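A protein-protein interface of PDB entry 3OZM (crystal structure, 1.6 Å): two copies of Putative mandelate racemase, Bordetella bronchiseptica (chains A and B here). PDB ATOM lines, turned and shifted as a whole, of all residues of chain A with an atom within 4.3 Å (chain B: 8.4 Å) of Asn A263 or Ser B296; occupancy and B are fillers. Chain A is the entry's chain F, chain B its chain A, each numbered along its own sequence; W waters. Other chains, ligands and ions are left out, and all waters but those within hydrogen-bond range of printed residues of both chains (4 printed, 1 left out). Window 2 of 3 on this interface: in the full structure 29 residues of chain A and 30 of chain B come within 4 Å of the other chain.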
ATOM      1  N   ARG A 259      21.441 -22.726 -10.916  1.00  0.00           N
ATOM      2  CA  ARG A 259      21.371 -23.531  -9.695  1.00  0.00           C
ATOM      3  C   ARG A 259      22.388 -24.662  -9.684  1.00  0.00           C
ATOM      4  O   ARG A 259      22.761 -25.152  -8.613  1.00  0.00           O
ATOM      5  CB  ARG A 259      19.961 -24.088  -9.501  1.00  0.00           C
ATOM      6  CG  ARG A 259      19.593 -25.168 -10.509  1.00  0.00           C
ATOM      7  CD  ARG A 259      18.116 -25.484 -10.416  1.00  0.00           C
ATOM      8  NE  ARG A 259      17.314 -24.488 -11.118  1.00  0.00           N
ATOM      9  CZ  ARG A 259      15.993 -24.405 -11.026  1.00  0.00           C
ATOM     10  NH1 ARG A 259      15.332 -25.240 -10.235  1.00  0.00           N
ATOM     11  NH2 ARG A 259      15.336 -23.475 -11.707  1.00  0.00           N
ATOM     12  N   ASN A 260      22.843 -25.075 -10.869  1.00  0.00           N
ATOM     13  CA  ASN A 260      23.753 -26.211 -10.993  1.00  0.00           C
ATOM     14  C   ASN A 260      25.110 -25.955 -10.353  1.00  0.00           C
ATOM     15  O   ASN A 260      25.703 -26.851  -9.743  1.00  0.00           O
ATOM     16  CB  ASN A 260      23.929 -26.588 -12.462  1.00  0.00           C
ATOM     17  CG  ASN A 260      22.609 -26.939 -13.124  1.00  0.00           C
ATOM     18  OD1 ASN A 260      21.951 -27.890 -12.725  1.00  0.00           O
ATOM     19  ND2 ASN A 260      22.205 -26.149 -14.116  1.00  0.00           N
ATOM     20  N   ALA A 261      25.616 -24.737 -10.515  1.00  0.00           N
ATOM     21  CA  ALA A 261      26.880 -24.370  -9.894  1.00  0.00           C
ATOM     22  C   ALA A 261      26.739 -24.476  -8.382  1.00  0.00           C
ATOM     23  O   ALA A 261      27.598 -25.015  -7.697  1.00  0.00           O
ATOM     24  CB  ALA A 261      27.278 -22.951 -10.282  1.00  0.00           C
ATOM     25  N   PHE A 262      25.645 -23.952  -7.862  1.00  0.00           N
ATOM     26  CA  PHE A 262      25.475 -23.891  -6.422  1.00  0.00           C
ATOM     27  C   PHE A 262      25.202 -25.278  -5.833  1.00  0.00           C
ATOM     28  O   PHE A 262      25.616 -25.585  -4.715  1.00  0.00           O
ATOM     29  CB  PHE A 262      24.421 -22.846  -6.061  1.00  0.00           C
ATOM     30  CG  PHE A 262      24.829 -21.451  -6.444  1.00  0.00           C
ATOM     31  CD1 PHE A 262      25.631 -20.690  -5.594  1.00  0.00           C
ATOM     32  CD2 PHE A 262      24.448 -20.903  -7.669  1.00  0.00           C
ATOM     33  CE1 PHE A 262      26.028 -19.399  -5.954  1.00  0.00           C
ATOM     34  CE2 PHE A 262      24.840 -19.634  -8.027  1.00  0.00           C
ATOM     35  CZ  PHE A 262      25.637 -18.873  -7.172  1.00  0.00           C
ATOM     36  N   ASN A 263      24.536 -26.128  -6.600  1.00  0.00           N
ATOM     37  CA  ASN A 263      24.347 -27.509  -6.172  1.00  0.00           C
ATOM     38  C   ASN A 263      25.696 -28.190  -5.973  1.00  0.00           C
ATOM     39  O   ASN A 263      25.906 -28.907  -4.990  1.00  0.00           O
ATOM     40  CB  ASN A 263      23.503 -28.281  -7.187  1.00  0.00           C
ATOM     41  CG  ASN A 263      23.322 -29.740  -6.808  1.00  0.00           C
ATOM     42  OD1 ASN A 263      23.763 -30.642  -7.529  1.00  0.00           O
ATOM     43  ND2 ASN A 263      22.664 -29.980  -5.684  1.00  0.00           N
ATOM     44  N   ASP A 264      26.628 -27.935  -6.890  1.00  0.00           N
ATOM     45  CA  ASP A 264      27.944 -28.551  -6.793  1.00  0.00           C
ATOM     46  C   ASP A 264      28.693 -28.086  -5.543  1.00  0.00           C
ATOM     47  O   ASP A 264      29.367 -28.879  -4.886  1.00  0.00           O
ATOM     48  CB  ASP A 264      28.761 -28.270  -8.052  1.00  0.00           C
ATOM     49  CG  ASP A 264      28.350 -29.151  -9.229  1.00  0.00           C
ATOM     50  OD1 ASP A 264      27.741 -30.226  -9.010  1.00  0.00           O
ATOM     51  OD2 ASP A 264      28.652 -28.779 -10.375  1.00  0.00           O
ATOM     52  N   TYR A 265      28.568 -26.806  -5.205  1.00  0.00           N
ATOM     53  CA  TYR A 265      29.153 -26.309  -3.959  1.00  0.00           C
ATOM     54  C   TYR A 265      28.482 -26.926  -2.730  1.00  0.00           C
ATOM     55  O   TYR A 265      29.161 -27.333  -1.792  1.00  0.00           O
ATOM     56  CB  TYR A 265      29.074 -24.780  -3.888  1.00  0.00           C
ATOM     57  CG  TYR A 265      30.293 -24.074  -4.474  1.00  0.00           C
ATOM     58  CD1 TYR A 265      30.471 -23.965  -5.842  1.00  0.00           C
ATOM     59  CD2 TYR A 265      31.269 -23.543  -3.644  1.00  0.00           C
ATOM     60  CE1 TYR A 265      31.589 -23.330  -6.375  1.00  0.00           C
ATOM     61  CE2 TYR A 265      32.380 -22.923  -4.159  1.00  0.00           C
ATOM     62  CZ  TYR A 265      32.535 -22.806  -5.519  1.00  0.00           C
ATOM     63  OH  TYR A 265      33.660 -22.185  -6.007  1.00  0.00           O
ATOM     64  N   ILE A 266      27.155 -26.982  -2.726  1.00  0.00           N
ATOM     65  CA  ILE A 266      26.430 -27.539  -1.590  1.00  0.00           C
ATOM     66  C   ILE A 266      26.784 -29.008  -1.390  1.00  0.00           C
ATOM     67  O   ILE A 266      27.058 -29.440  -0.270  1.00  0.00           O
ATOM     68  CB  ILE A 266      24.900 -27.367  -1.755  1.00  0.00           C
ATOM     69  CG1 ILE A 266      24.528 -25.886  -1.667  1.00  0.00           C
ATOM     70  CG2 ILE A 266      24.126 -28.164  -0.698  1.00  0.00           C
ATOM     71  CD1 ILE A 266      23.082 -25.612  -2.011  1.00  0.00           C
ATOM     72  N   ARG A 267      26.784 -29.768  -2.482  1.00  0.00           N
ATOM     73  CA  ARG A 267      27.118 -31.195  -2.458  1.00  0.00           C
ATOM     74  C   ARG A 267      28.498 -31.451  -1.879  1.00  0.00           C
ATOM     75  O   ARG A 267      28.767 -32.528  -1.349  1.00  0.00           O
ATOM     76  CB  ARG A 267      27.089 -31.787  -3.871  1.00  0.00           C
ATOM     77  CG  ARG A 267      25.719 -32.153  -4.388  1.00  0.00           C
ATOM     78  CD  ARG A 267      25.855 -32.912  -5.713  1.00  0.00           C
ATOM     79  NE  ARG A 267      26.958 -32.406  -6.534  1.00  0.00           N
ATOM     80  CZ  ARG A 267      27.841 -33.185  -7.155  1.00  0.00           C
ATOM     81  NH1 ARG A 267      27.743 -34.506  -7.046  1.00  0.00           N
ATOM     82  NH2 ARG A 267      28.822 -32.653  -7.879  1.00  0.00           N
ATOM     83  N   SER A 293      16.703 -23.623  -2.706  1.00  0.00           N
ATOM     84  CA  SER A 293      17.657 -24.713  -2.558  1.00  0.00           C
ATOM     85  C   SER A 293      18.642 -24.450  -1.412  1.00  0.00           C
ATOM     86  O   SER A 293      19.053 -25.375  -0.714  1.00  0.00           O
ATOM     87  CB  SER A 293      18.389 -24.977  -3.874  1.00  0.00           C
ATOM     88  OG  SER A 293      17.469 -25.400  -4.866  1.00  0.00           O
ATOM     89  N   ILE B 266      17.430 -36.671   0.125  1.00  0.00           N
ATOM     90  CA  ILE B 266      18.387 -36.328  -0.925  1.00  0.00           C
ATOM     91  C   ILE B 266      19.827 -36.490  -0.443  1.00  0.00           C
ATOM     92  O   ILE B 266      20.662 -37.063  -1.148  1.00  0.00           O
ATOM     93  CB  ILE B 266      18.142 -34.909  -1.454  1.00  0.00           C
ATOM     94  CG1 ILE B 266      16.833 -34.877  -2.224  1.00  0.00           C
ATOM     95  CG2 ILE B 266      19.273 -34.472  -2.385  1.00  0.00           C
ATOM     96  CD1 ILE B 266      16.368 -33.481  -2.546  1.00  0.00           C
ATOM     97  N   ALA B 289       9.181 -24.564  -2.972  1.00  0.00           N
ATOM     98  CA  ALA B 289      10.567 -24.727  -2.546  1.00  0.00           C
ATOM     99  C   ALA B 289      11.091 -26.148  -2.754  1.00  0.00           C
ATOM    100  O   ALA B 289      12.240 -26.346  -3.149  1.00  0.00           O
ATOM    101  CB  ALA B 289      10.734 -24.293  -1.093  1.00  0.00           C
ATOM    102  N   ILE B 290      10.243 -27.133  -2.476  1.00  0.00           N
ATOM    103  CA  ILE B 290      10.608 -28.534  -2.658  1.00  0.00           C
ATOM    104  C   ILE B 290      10.819 -28.854  -4.136  1.00  0.00           C
ATOM    105  O   ILE B 290      11.794 -29.489  -4.502  1.00  0.00           O
ATOM    106  CB  ILE B 290       9.568 -29.456  -2.010  1.00  0.00           C
ATOM    107  CG1 ILE B 290       9.586 -29.238  -0.491  1.00  0.00           C
ATOM    108  CG2 ILE B 290       9.846 -30.920  -2.338  1.00  0.00           C
ATOM    109  CD1 ILE B 290       8.408 -29.853   0.263  1.00  0.00           C
ATOM    110  N   SER B 291       9.919 -28.374  -4.985  1.00  0.00           N
ATOM    111  CA  SER B 291      10.070 -28.527  -6.431  1.00  0.00           C
ATOM    112  C   SER B 291      11.411 -27.961  -6.929  1.00  0.00           C
ATOM    113  O   SER B 291      12.123 -28.594  -7.735  1.00  0.00           O
ATOM    114  CB  SER B 291       8.898 -27.857  -7.158  1.00  0.00           C
ATOM    115  OG  SER B 291       9.078 -27.930  -8.560  1.00  0.00           O
ATOM    116  N   ALA B 292      11.772 -26.776  -6.442  1.00  0.00           N
ATOM    117  CA  ALA B 292      13.032 -26.157  -6.838  1.00  0.00           C
ATOM    118  C   ALA B 292      14.224 -26.961  -6.347  1.00  0.00           C
ATOM    119  O   ALA B 292      15.198 -27.159  -7.087  1.00  0.00           O
ATOM    120  CB  ALA B 292      13.120 -24.741  -6.312  1.00  0.00           C
ATOM    121  N   SER B 293      14.158 -27.399  -5.093  1.00  0.00           N
ATOM    122  CA  SER B 293      15.228 -28.182  -4.489  1.00  0.00           C
ATOM    123  C   SER B 293      15.430 -29.516  -5.207  1.00  0.00           C
ATOM    124  O   SER B 293      16.564 -29.943  -5.419  1.00  0.00           O
ATOM    125  CB  SER B 293      14.953 -28.400  -3.000  1.00  0.00           C
ATOM    126  OG  SER B 293      14.930 -27.156  -2.312  1.00  0.00           O
ATOM    127  N   ALA B 294      14.333 -30.165  -5.590  1.00  0.00           N
ATOM    128  CA  ALA B 294      14.412 -31.380  -6.401  1.00  0.00           C
ATOM    129  C   ALA B 294      15.182 -31.112  -7.689  1.00  0.00           C
ATOM    130  O   ALA B 294      16.065 -31.880  -8.057  1.00  0.00           O
ATOM    131  CB  ALA B 294      13.039 -31.908  -6.732  1.00  0.00           C
ATOM    132  N   ALA B 295      14.833 -30.027  -8.379  1.00  0.00           N
ATOM    133  CA  ALA B 295      15.482 -29.699  -9.643  1.00  0.00           C
ATOM    134  C   ALA B 295      16.977 -29.430  -9.466  1.00  0.00           C
ATOM    135  O   ALA B 295      17.794 -29.860 -10.280  1.00  0.00           O
ATOM    136  CB  ALA B 295      14.807 -28.503 -10.286  1.00  0.00           C
ATOM    137  N   SER B 296      17.327 -28.683  -8.422  1.00  0.00           N
ATOM    138  CA  SER B 296      18.729 -28.403  -8.139  1.00  0.00           C
ATOM    139  C   SER B 296      19.543 -29.682  -7.989  1.00  0.00           C
ATOM    140  O   SER B 296      20.709 -29.732  -8.383  1.00  0.00           O
ATOM    141  CB  SER B 296      18.875 -27.571  -6.862  1.00  0.00           C
ATOM    142  OG  SER B 296      18.414 -26.254  -7.056  1.00  0.00           O
ATOM    143  N   ALA B 297      18.924 -30.707  -7.406  1.00  0.00           N
ATOM    144  CA  ALA B 297      19.580 -31.990  -7.193  1.00  0.00           C
ATOM    145  C   ALA B 297      19.456 -32.955  -8.383  1.00  0.00           C
ATOM    146  O   ALA B 297      19.867 -34.114  -8.285  1.00  0.00           O
ATOM    147  CB  ALA B 297      19.020 -32.650  -5.926  1.00  0.00           C
ATOM    148  N   HIS B 298      18.889 -32.476  -9.492  1.00  0.00           N
ATOM    149  CA  HIS B 298      18.643 -33.294 -10.698  1.00  0.00           C
ATOM    150  C   HIS B 298      17.696 -34.463 -10.435  1.00  0.00           C
ATOM    151  O   HIS B 298      17.830 -35.547 -11.017  1.00  0.00           O
ATOM    152  CB  HIS B 298      19.962 -33.756 -11.338  1.00  0.00           C
ATOM    153  CG  HIS B 298      20.872 -32.617 -11.655  1.00  0.00           C
ATOM    154  ND1 HIS B 298      20.783 -31.904 -12.829  1.00  0.00           N
ATOM    155  CD2 HIS B 298      21.834 -32.013 -10.916  1.00  0.00           C
ATOM    156  CE1 HIS B 298      21.676 -30.931 -12.818  1.00  0.00           C
ATOM    157  NE2 HIS B 298      22.327 -30.976 -11.669  1.00  0.00           N
ATOM    158  N   LEU B 299      16.745 -34.225  -9.540  1.00  0.00           N
ATOM    159  CA  LEU B 299      15.708 -35.205  -9.206  1.00  0.00           C
ATOM    160  C   LEU B 299      14.358 -34.655  -9.659  1.00  0.00           C
ATOM    161  O   LEU B 299      14.295 -33.541 -10.152  1.00  0.00           O
ATOM    162  CB  LEU B 299      15.689 -35.466  -7.702  1.00  0.00           C
ATOM    163  CG  LEU B 299      17.040 -35.927  -7.148  1.00  0.00           C
ATOM    164  CD1 LEU B 299      16.965 -36.094  -5.640  1.00  0.00           C
ATOM    165  CD2 LEU B 299      17.462 -37.238  -7.811  1.00  0.00           C
ATOM    166  N   ALA B 300      13.282 -35.422  -9.479  1.00  0.00           N
ATOM    167  CA  ALA B 300      11.960 -34.989  -9.967  1.00  0.00           C
ATOM    168  C   ALA B 300      11.029 -34.650  -8.822  1.00  0.00           C
ATOM    169  O   ALA B 300      11.139 -35.226  -7.746  1.00  0.00           O
ATOM    170  CB  ALA B 300      11.334 -36.089 -10.838  1.00  0.00           C
ATOM    171  N   HIS B 324       9.552 -29.846 -14.277  1.00  0.00           N
ATOM    172  CA  HIS B 324       9.627 -31.299 -14.061  1.00  0.00           C
ATOM    173  C   HIS B 324       8.694 -32.007 -15.040  1.00  0.00           C
ATOM    174  O   HIS B 324       7.527 -31.624 -15.169  1.00  0.00           O
ATOM    175  CB  HIS B 324       9.203 -31.661 -12.637  1.00  0.00           C
ATOM    176  CG  HIS B 324      10.160 -31.203 -11.581  1.00  0.00           C
ATOM    177  ND1 HIS B 324      11.427 -31.729 -11.447  1.00  0.00           N
ATOM    178  CD2 HIS B 324      10.035 -30.265 -10.612  1.00  0.00           C
ATOM    179  CE1 HIS B 324      12.040 -31.134 -10.440  1.00  0.00           C
ATOM    180  NE2 HIS B 324      11.219 -30.239  -9.919  1.00  0.00           N
HETATM  181  O   HOH W   1      21.287 -25.055  -6.043  1.00  0.00           O
HETATM  182  O   HOH W   2      21.207 -28.284 -10.381  1.00  0.00           O
HETATM  183  O   HOH W   3      23.257 -33.659  -7.941  1.00  0.00           O
HETATM  184  O   HOH W   4      19.070 -28.239 -12.599  1.00  0.00           O
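Among the printed residues, merely in contact across the chains: Arg A259 with Ala B292, Arg A259 with Ala B295, Arg A259 with Ser B296, Asn A263 with Ala B297, Ser A293 with Ala B292 and Ser A293 with Ser B293.
The backbone carbonyl oxygen (O) of Ser B296 sits close to the side-chain amide oxygen (OD1) of Asn A263 (3.3 Å).
The side-chain hydroxyl (OG) of Ser A293 is in hydrogen-bond range of the side-chain hydroxyl (OG) of Ser B296 (2.5 Å).
A ring nitrogen (NE2) of His B298 lies close to the side-chain amide oxygen (OD1) of Asn A260, at 3.3 Å.
Ser B293 touches its own counterpart, Ser A293.
Positions printed for both chains: 266 and 293.
Of the 9 pairs that touch across the chains among the printed residues, 1 has its exchanged pair printed and touching as well.
Water W2 lies within hydrogen-bond range of the side-chain amide oxygen (OD1) of Asn A260, the backbone carbonyl oxygen (O) of Ser B296 and a ring nitrogen (NE2) of His B298.
Water W4 lies within hydrogen-bond range of OD1 of Asn A260 (2.9 Å) and O of Ala B295 (3.1 Å).
Water W1 lies within hydrogen-bond range of O of Arg A259 (3.0 Å), OG of Ser B296 (3.3 Å) and N of Asn A263 (3.5 Å).
Water W3 bridges the side-chain amide oxygen of Asn A263 (3.1 Å) and the backbone carbonyl oxygen of Ala B297 (3.4 Å).
Of the 10 printed residues of chain A, 4 touch a printed residue of chain B.
Printed residues of chain A that touch a printed residue of chain B: Arg A259, Asn A260, Asn A263 and Ser A293.
Along chain A the printed residues that touch a printed residue of chain B span positions 259 to 293.
Among the printed residues, 9 pairs touch across the chains.
The backbone carbonyl oxygen (O) of Ala B289 lies within hydrogen-bond range of the side-chain hydroxyl (OG) of Ser B293, 2.9 Å away.
O of Ala B292 is in hydrogen-bond range of OG of Ser B296 (3.3 Å).
Asn A263 touches two residues of chain B.
Of the printed residues of chain A, Ser B296 touches Arg A259 (3.5 Å), Asn A263 (3.1 Å) and Ser A293 (2.5 Å).
Of the printed residues of chain B, Arg A259 touches Ala B292, Ala B295 and Ser B296.
Of the printed residues of chain B, Asn A260 touches His B298.
Of the printed residues of chain B, Ser A293 touches Ala B292, Ser B293 and Ser B296.
Of the printed residues of chain A, His B298 touches Asn A260.
Of the printed residues of chain A, Ala B297 touches Asn A263 (3.98 Å).
Phe A262 touches none of the printed residues of chain B.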
